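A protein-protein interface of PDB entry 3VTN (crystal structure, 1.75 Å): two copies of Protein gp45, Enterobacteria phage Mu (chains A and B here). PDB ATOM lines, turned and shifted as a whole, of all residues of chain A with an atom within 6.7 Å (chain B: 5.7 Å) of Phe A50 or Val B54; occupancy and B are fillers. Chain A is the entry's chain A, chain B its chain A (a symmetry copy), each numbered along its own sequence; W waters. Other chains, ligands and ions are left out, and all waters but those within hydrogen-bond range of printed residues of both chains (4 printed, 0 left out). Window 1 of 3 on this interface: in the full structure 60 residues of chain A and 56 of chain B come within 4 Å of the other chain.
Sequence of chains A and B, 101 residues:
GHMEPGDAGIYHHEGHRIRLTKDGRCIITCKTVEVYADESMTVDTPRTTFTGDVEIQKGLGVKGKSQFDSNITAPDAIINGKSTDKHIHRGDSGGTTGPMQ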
ATOM      1  N   PRO A  46     -16.324  -0.330  23.273  1.00  0.00           N
ATOM      2  CA  PRO A  46     -17.541   0.275  22.758  1.00  0.00           C
ATOM      3  C   PRO A  46     -17.568   1.768  22.898  1.00  0.00           C
ATOM      4  O   PRO A  46     -18.213   2.451  22.048  1.00  0.00           O
ATOM      5  CB  PRO A  46     -18.637  -0.362  23.590  1.00  0.00           C
ATOM      6  CG  PRO A  46     -18.042  -1.675  24.000  1.00  0.00           C
ATOM      7  CD  PRO A  46     -16.591  -1.471  24.155  1.00  0.00           C
ATOM      8  N   ARG A  47     -16.954   2.288  23.972  1.00  0.00           N
ATOM      9  CA  ARG A  47     -16.956   3.749  24.185  1.00  0.00           C
ATOM     10  C   ARG A  47     -15.712   4.204  24.948  1.00  0.00           C
ATOM     11  O   ARG A  47     -15.364   3.649  26.001  1.00  0.00           O
ATOM     12  CB  ARG A  47     -18.178   4.112  25.071  1.00  0.00           C
ATOM     13  CG  ARG A  47     -18.299   5.586  25.277  1.00  0.00           C
ATOM     14  CD  ARG A  47     -19.692   5.910  25.776  1.00  0.00           C
ATOM     15  NE  ARG A  47     -19.963   7.307  25.498  1.00  0.00           N
ATOM     16  CZ  ARG A  47     -20.512   7.810  24.397  1.00  0.00           C
ATOM     17  NH1 ARG A  47     -20.984   7.047  23.402  1.00  0.00           N
ATOM     18  NH2 ARG A  47     -20.709   9.110  24.355  1.00  0.00           N
ATOM     19  N   THR A  48     -15.034   5.194  24.379  1.00  0.00           N
ATOM     20  CA  THR A  48     -13.887   5.850  24.993  1.00  0.00           C
ATOM     21  C   THR A  48     -14.268   7.270  25.306  1.00  0.00           C
ATOM     22  O   THR A  48     -14.695   8.017  24.403  1.00  0.00           O
ATOM     23  CB  THR A  48     -12.666   5.891  24.026  1.00  0.00           C
ATOM     24  OG1 THR A  48     -12.335   4.549  23.601  1.00  0.00           O
ATOM     25  CG2 THR A  48     -11.460   6.455  24.763  1.00  0.00           C
ATOM     26  N   THR A  49     -13.973   7.690  26.535  1.00  0.00           N
ATOM     27  CA  THR A  49     -14.335   9.064  26.959  1.00  0.00           C
ATOM     28  C   THR A  49     -13.095   9.778  27.430  1.00  0.00           C
ATOM     29  O   THR A  49     -12.363   9.250  28.276  1.00  0.00           O
ATOM     30  CB  THR A  49     -15.340   8.997  28.119  1.00  0.00           C
ATOM     31  OG1 THR A  49     -16.516   8.385  27.650  1.00  0.00           O
ATOM     32  CG2 THR A  49     -15.727  10.395  28.596  1.00  0.00           C
ATOM     33  N   PHE A  50     -12.872  10.970  26.859  1.00  0.00           N
ATOM     34  CA  PHE A  50     -11.821  11.892  27.306  1.00  0.00           C
ATOM     35  C   PHE A  50     -12.467  13.007  28.111  1.00  0.00           C
ATOM     36  O   PHE A  50     -13.324  13.719  27.613  1.00  0.00           O
ATOM     37  CB  PHE A  50     -11.085  12.488  26.084  1.00  0.00           C
ATOM     38  CG  PHE A  50     -10.406  11.443  25.245  1.00  0.00           C
ATOM     39  CD1 PHE A  50      -9.113  10.979  25.617  1.00  0.00           C
ATOM     40  CD2 PHE A  50     -11.075  10.815  24.189  1.00  0.00           C
ATOM     41  CE1 PHE A  50      -8.471   9.984  24.916  1.00  0.00           C
ATOM     42  CE2 PHE A  50     -10.456   9.738  23.489  1.00  0.00           C
ATOM     43  CZ  PHE A  50      -9.157   9.323  23.851  1.00  0.00           C
ATOM     44  N   THR A  51     -11.993  13.209  29.324  1.00  0.00           N
ATOM     45  CA  THR A  51     -12.653  14.225  30.183  1.00  0.00           C
ATOM     46  C   THR A  51     -12.211  15.615  29.866  1.00  0.00           C
ATOM     47  O   THR A  51     -12.879  16.585  30.286  1.00  0.00           O
ATOM     48  CB  THR A  51     -12.409  13.952  31.674  1.00  0.00           C
ATOM     49  OG1 THR A  51     -11.029  14.111  31.981  1.00  0.00           O
ATOM     50  CG2 THR A  51     -12.880  12.585  32.046  1.00  0.00           C
ATOM     51  N   GLY A  52     -11.074  15.724  29.165  1.00  0.00           N
ATOM     52  CA  GLY A  52     -10.533  17.023  28.898  1.00  0.00           C
ATOM     53  C   GLY A  52     -10.478  17.353  27.429  1.00  0.00           C
ATOM     54  O   GLY A  52     -11.283  16.904  26.625  1.00  0.00           O
ATOM     55  N   ASP A  53      -9.512  18.198  27.085  1.00  0.00           N
ATOM     56  CA  ASP A  53      -9.278  18.562  25.701  1.00  0.00           C
ATOM     57  C   ASP A  53      -8.491  17.477  24.973  1.00  0.00           C
ATOM     58  O   ASP A  53      -7.774  16.688  25.616  1.00  0.00           O
ATOM     59  CB  ASP A  53      -8.452  19.842  25.696  1.00  0.00           C
ATOM     60  CG  ASP A  53      -9.248  21.033  26.168  1.00  0.00           C
ATOM     61  OD1 ASP A  53     -10.099  21.457  25.426  1.00  0.00           O
ATOM     62  OD2 ASP A  53      -9.059  21.511  27.286  1.00  0.00           O
ATOM     63  N   VAL A  54      -8.568  17.483  23.642  1.00  0.00           N
ATOM     64  CA  VAL A  54      -7.849  16.483  22.830  1.00  0.00           C
ATOM     65  C   VAL A  54      -7.255  17.268  21.665  1.00  0.00           C
ATOM     66  O   VAL A  54      -7.958  18.136  21.096  1.00  0.00           O
ATOM     67  CB  VAL A  54      -8.822  15.416  22.265  1.00  0.00           C
ATOM     68  CG1 VAL A  54      -8.067  14.440  21.364  1.00  0.00           C
ATOM     69  CG2 VAL A  54      -9.429  14.615  23.388  1.00  0.00           C
ATOM     70  N   PHE B  50      -9.823   3.865  17.262  1.00  0.00           N
ATOM     71  CA  PHE B  50     -10.872   3.529  18.233  1.00  0.00           C
ATOM     72  C   PHE B  50     -11.955   2.737  17.519  1.00  0.00           C
ATOM     73  O   PHE B  50     -12.547   3.212  16.563  1.00  0.00           O
ATOM     74  CB  PHE B  50     -11.477   4.821  18.829  1.00  0.00           C
ATOM     75  CG  PHE B  50     -10.465   5.652  19.566  1.00  0.00           C
ATOM     76  CD1 PHE B  50     -10.158   5.342  20.921  1.00  0.00           C
ATOM     77  CD2 PHE B  50      -9.717   6.633  18.907  1.00  0.00           C
ATOM     78  CE1 PHE B  50      -9.201   6.035  21.624  1.00  0.00           C
ATOM     79  CE2 PHE B  50      -8.674   7.321  19.597  1.00  0.00           C
ATOM     80  CZ  PHE B  50      -8.416   7.023  20.952  1.00  0.00           C
ATOM     81  N   GLY B  52     -14.853   1.899  18.672  1.00  0.00           N
ATOM     82  CA  GLY B  52     -16.186   2.260  19.054  1.00  0.00           C
ATOM     83  C   GLY B  52     -16.442   3.742  18.987  1.00  0.00           C
ATOM     84  O   GLY B  52     -15.870   4.472  18.190  1.00  0.00           O
ATOM     85  N   ASP B  53     -17.364   4.186  19.836  1.00  0.00           N
ATOM     86  CA  ASP B  53     -17.678   5.596  19.949  1.00  0.00           C
ATOM     87  C   ASP B  53     -16.643   6.322  20.804  1.00  0.00           C
ATOM     88  O   ASP B  53     -15.968   5.690  21.638  1.00  0.00           O
ATOM     89  CB  ASP B  53     -19.034   5.713  20.631  1.00  0.00           C
ATOM     90  CG  ASP B  53     -20.159   5.248  19.741  1.00  0.00           C
ATOM     91  OD1 ASP B  53     -20.453   5.953  18.808  1.00  0.00           O
ATOM     92  OD2 ASP B  53     -20.712   4.166  19.942  1.00  0.00           O
ATOM     93  N   VAL B  54     -16.571   7.645  20.650  1.00  0.00           N
ATOM     94  CA  VAL B  54     -15.611   8.454  21.423  1.00  0.00           C
ATOM     95  C   VAL B  54     -16.391   9.689  21.861  1.00  0.00           C
ATOM     96  O   VAL B  54     -17.149  10.253  21.038  1.00  0.00           O
ATOM     97  CB  VAL B  54     -14.420   8.906  20.539  1.00  0.00           C
ATOM     98  CG1 VAL B  54     -13.482   9.807  21.341  1.00  0.00           C
ATOM     99  CG2 VAL B  54     -13.620   7.712  20.088  1.00  0.00           C
ATOM    100  N   GLU B  55     -16.249  10.078  23.120  1.00  0.00           N
ATOM    101  CA  GLU B  55     -16.743  11.412  23.577  1.00  0.00           C
ATOM    102  C   GLU B  55     -15.576  12.227  24.068  1.00  0.00           C
ATOM    103  O   GLU B  55     -14.766  11.712  24.868  1.00  0.00           O
ATOM    104  CB  GLU B  55     -17.719  11.263  24.729  1.00  0.00           C
ATOM    105  CG  GLU B  55     -18.186  12.595  25.275  1.00  0.00           C
ATOM    106  CD  GLU B  55     -19.274  12.503  26.400  1.00  0.00           C
ATOM    107  OE1 GLU B  55     -19.553  11.433  26.915  1.00  0.00           O
ATOM    108  OE2 GLU B  55     -19.864  13.540  26.756  1.00  0.00           O
ATOM    109  N   ILE B  56     -15.506  13.506  23.631  1.00  0.00           N
ATOM    110  CA  ILE B  56     -14.524  14.455  24.159  1.00  0.00           C
ATOM    111  C   ILE B  56     -15.288  15.482  24.954  1.00  0.00           C
ATOM    112  O   ILE B  56     -16.151  16.122  24.388  1.00  0.00           O
ATOM    113  CB  ILE B  56     -13.742  15.104  23.027  1.00  0.00           C
ATOM    114  CG1 ILE B  56     -13.009  13.993  22.297  1.00  0.00           C
ATOM    115  CG2 ILE B  56     -12.708  16.141  23.536  1.00  0.00           C
ATOM    116  CD1 ILE B  56     -12.327  14.460  20.986  1.00  0.00           C
ATOM    117  N   GLN B  57     -14.935  15.632  26.223  1.00  0.00           N
ATOM    118  CA  GLN B  57     -15.767  16.417  27.156  1.00  0.00           C
ATOM    119  C   GLN B  57     -15.320  17.849  27.279  1.00  0.00           C
ATOM    120  O   GLN B  57     -16.062  18.670  27.828  1.00  0.00           O
ATOM    121  CB  GLN B  57     -15.875  15.739  28.527  1.00  0.00           C
ATOM    122  CG  GLN B  57     -16.599  14.370  28.394  1.00  0.00           C
ATOM    123  CD  GLN B  57     -16.839  13.715  29.711  1.00  0.00           C
ATOM    124  OE1 GLN B  57     -16.116  13.946  30.676  1.00  0.00           O
ATOM    125  NE2 GLN B  57     -17.883  12.902  29.781  1.00  0.00           N
ATOM    126  N   LYS B  58     -14.137  18.175  26.766  1.00  0.00           N
ATOM    127  CA  LYS B  58     -13.819  19.589  26.531  1.00  0.00           C
ATOM    128  C   LYS B  58     -13.705  19.838  25.039  1.00  0.00           C
ATOM    129  O   LYS B  58     -14.601  19.491  24.299  1.00  0.00           O
ATOM    130  CB  LYS B  58     -12.587  20.081  27.327  1.00  0.00           C
ATOM    131  CG  LYS B  58     -12.603  19.906  28.864  1.00  0.00           C
ATOM    132  CD  LYS B  58     -13.473  20.842  29.598  1.00  0.00           C
ATOM    133  CE  LYS B  58     -13.403  20.488  31.082  1.00  0.00           C
ATOM    134  NZ  LYS B  58     -14.236  21.423  31.904  1.00  0.00           N
HETATM  135  O   HOH W   1     -20.023  10.126  22.035  1.00  0.00           O
HETATM  136  O   HOH W   2     -14.909  16.832  32.040  1.00  0.00           O
HETATM  137  O   HOH W   3     -18.985   8.952  27.267  1.00  0.00           O
HETATM  138  O   HOH W   4     -14.118   3.494  21.372  1.00  0.00           O
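N of Asp B53 is in hydrogen-bond range of O of Pro A46 (2.9 Å).
NH2 of Arg A47 lies within salt-bridge range of OE1 of Glu B55, 3.6 Å away.
N of Thr A48 lies within hydrogen-bond range of O of Asp B53 (2.9 Å).
N of Glu B55 sits at hydrogen-bond distance from O of Thr A48 (2.9 Å).
The backbone NH (N) of Phe A50 is in hydrogen-bond range of the backbone carbonyl oxygen (O) of Glu B55 (2.8 Å).
The backbone carbonyl oxygen (O) of Phe A50 is in hydrogen-bond range of the backbone NH (N) of Gln B57 (2.9 Å).
O of Gly A52 lies within hydrogen-bond range of N of Lys B58.
O of Pro A46 touches CA of Gly B52 (3.6 Å).
Asp B53 touches Arg A47.
OG1 of Thr A48 touches CD1 of Phe B50 (3.5 Å).
CZ of Phe A50 touches CZ of Phe B50 (3.8 Å).
Phe A50 touches Val B54 (CE2 to CG1, 3.7 Å).
CA of Ile B56 touches O of Phe A50, 3.7 Å away.
Thr A51 touches Gln B57.
Lys B58 touches Thr A51.
Gly A52 touches Ile B56 (O to CG2, 3.5 Å).
Gly A52 touches Gln B57.
Printed residues of chain B within 4 Å of Thr A48: Phe B50 (3.5 Å), Asp B53 (2.9 Å), Val B54 (3.1 Å) and Glu B55 (2.9 Å).
Of chain B, only Phe B50, Val B54, Glu B55, Ile B56 and Gln B57 come within 4 Å of Phe A50.
Printed residues of chain B within 4 Å of Val A54: Ile B56 (3.6 Å).
Of the printed residues of chain A, Phe B50 touches Thr A48 (3.5 Å) and Phe A50 (3.8 Å).
Of chain A, only Thr A48 and Phe A50 come within 4 Å of Val B54.
Of the printed residues of chain A, Ile B56 touches Phe A50, Gly A52 and Val A54.
Of the printed residues of chain A, Gln B57 touches Thr A49 (3.5 Å), Phe A50 (2.9 Å), Thr A51 (3.5 Å) and Gly A52 (3.9 Å).
The nearest residue of chain B that does not touch Phe A50 is Lys B58 (4.6 Å).
The nearest residue of chain A that does not touch Val B54 is Arg A47 (5.0 Å).
Of the 8 printed residues of chain B, 8 touch a printed residue of chain A.
Hydrophobic or aromatic side chains of chain B that line the printed part of chain A: Phe B50, Val B54 and Ile B56.
Of the 9 printed residues of chain A, 9 touch a printed residue of chain B.
Hydrophobic or aromatic side chains of chain A within 4 Å of the printed part of chain B: Phe A50 and Val A54.
Phe B50 touches its own counterpart, Phe A50.
Phe A50 touches Val B54, but with the chains exchanged Val A54 does not touch Phe B50 (7.4 Å).
Positions printed for both chains: 50, 52, 53 and 54.
Of the 22 pairs that touch across the chains among the printed residues, 1 has its exchanged pair printed and touching as well.
Water W3 lies within hydrogen-bond range of the side-chain hydroxyl of Thr A49 (2.6 Å), the side-chain carboxylate of Glu B55 (2.6 Å) and the guanidinium group of Arg A47 (2.6 Å).
Water W1 lies within hydrogen-bond range of NH2 of Arg A47 and O of Val B54.
Water W2 lies within hydrogen-bond range of the backbone carbonyl oxygen of Thr A51 and the side-chain amide oxygen of Gln B57.
Water W4 lies within hydrogen-bond range of O of Asp B53 (2.9 Å), OG1 of Thr A48 (3.0 Å) and N of Gly B52 (3.2 Å).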
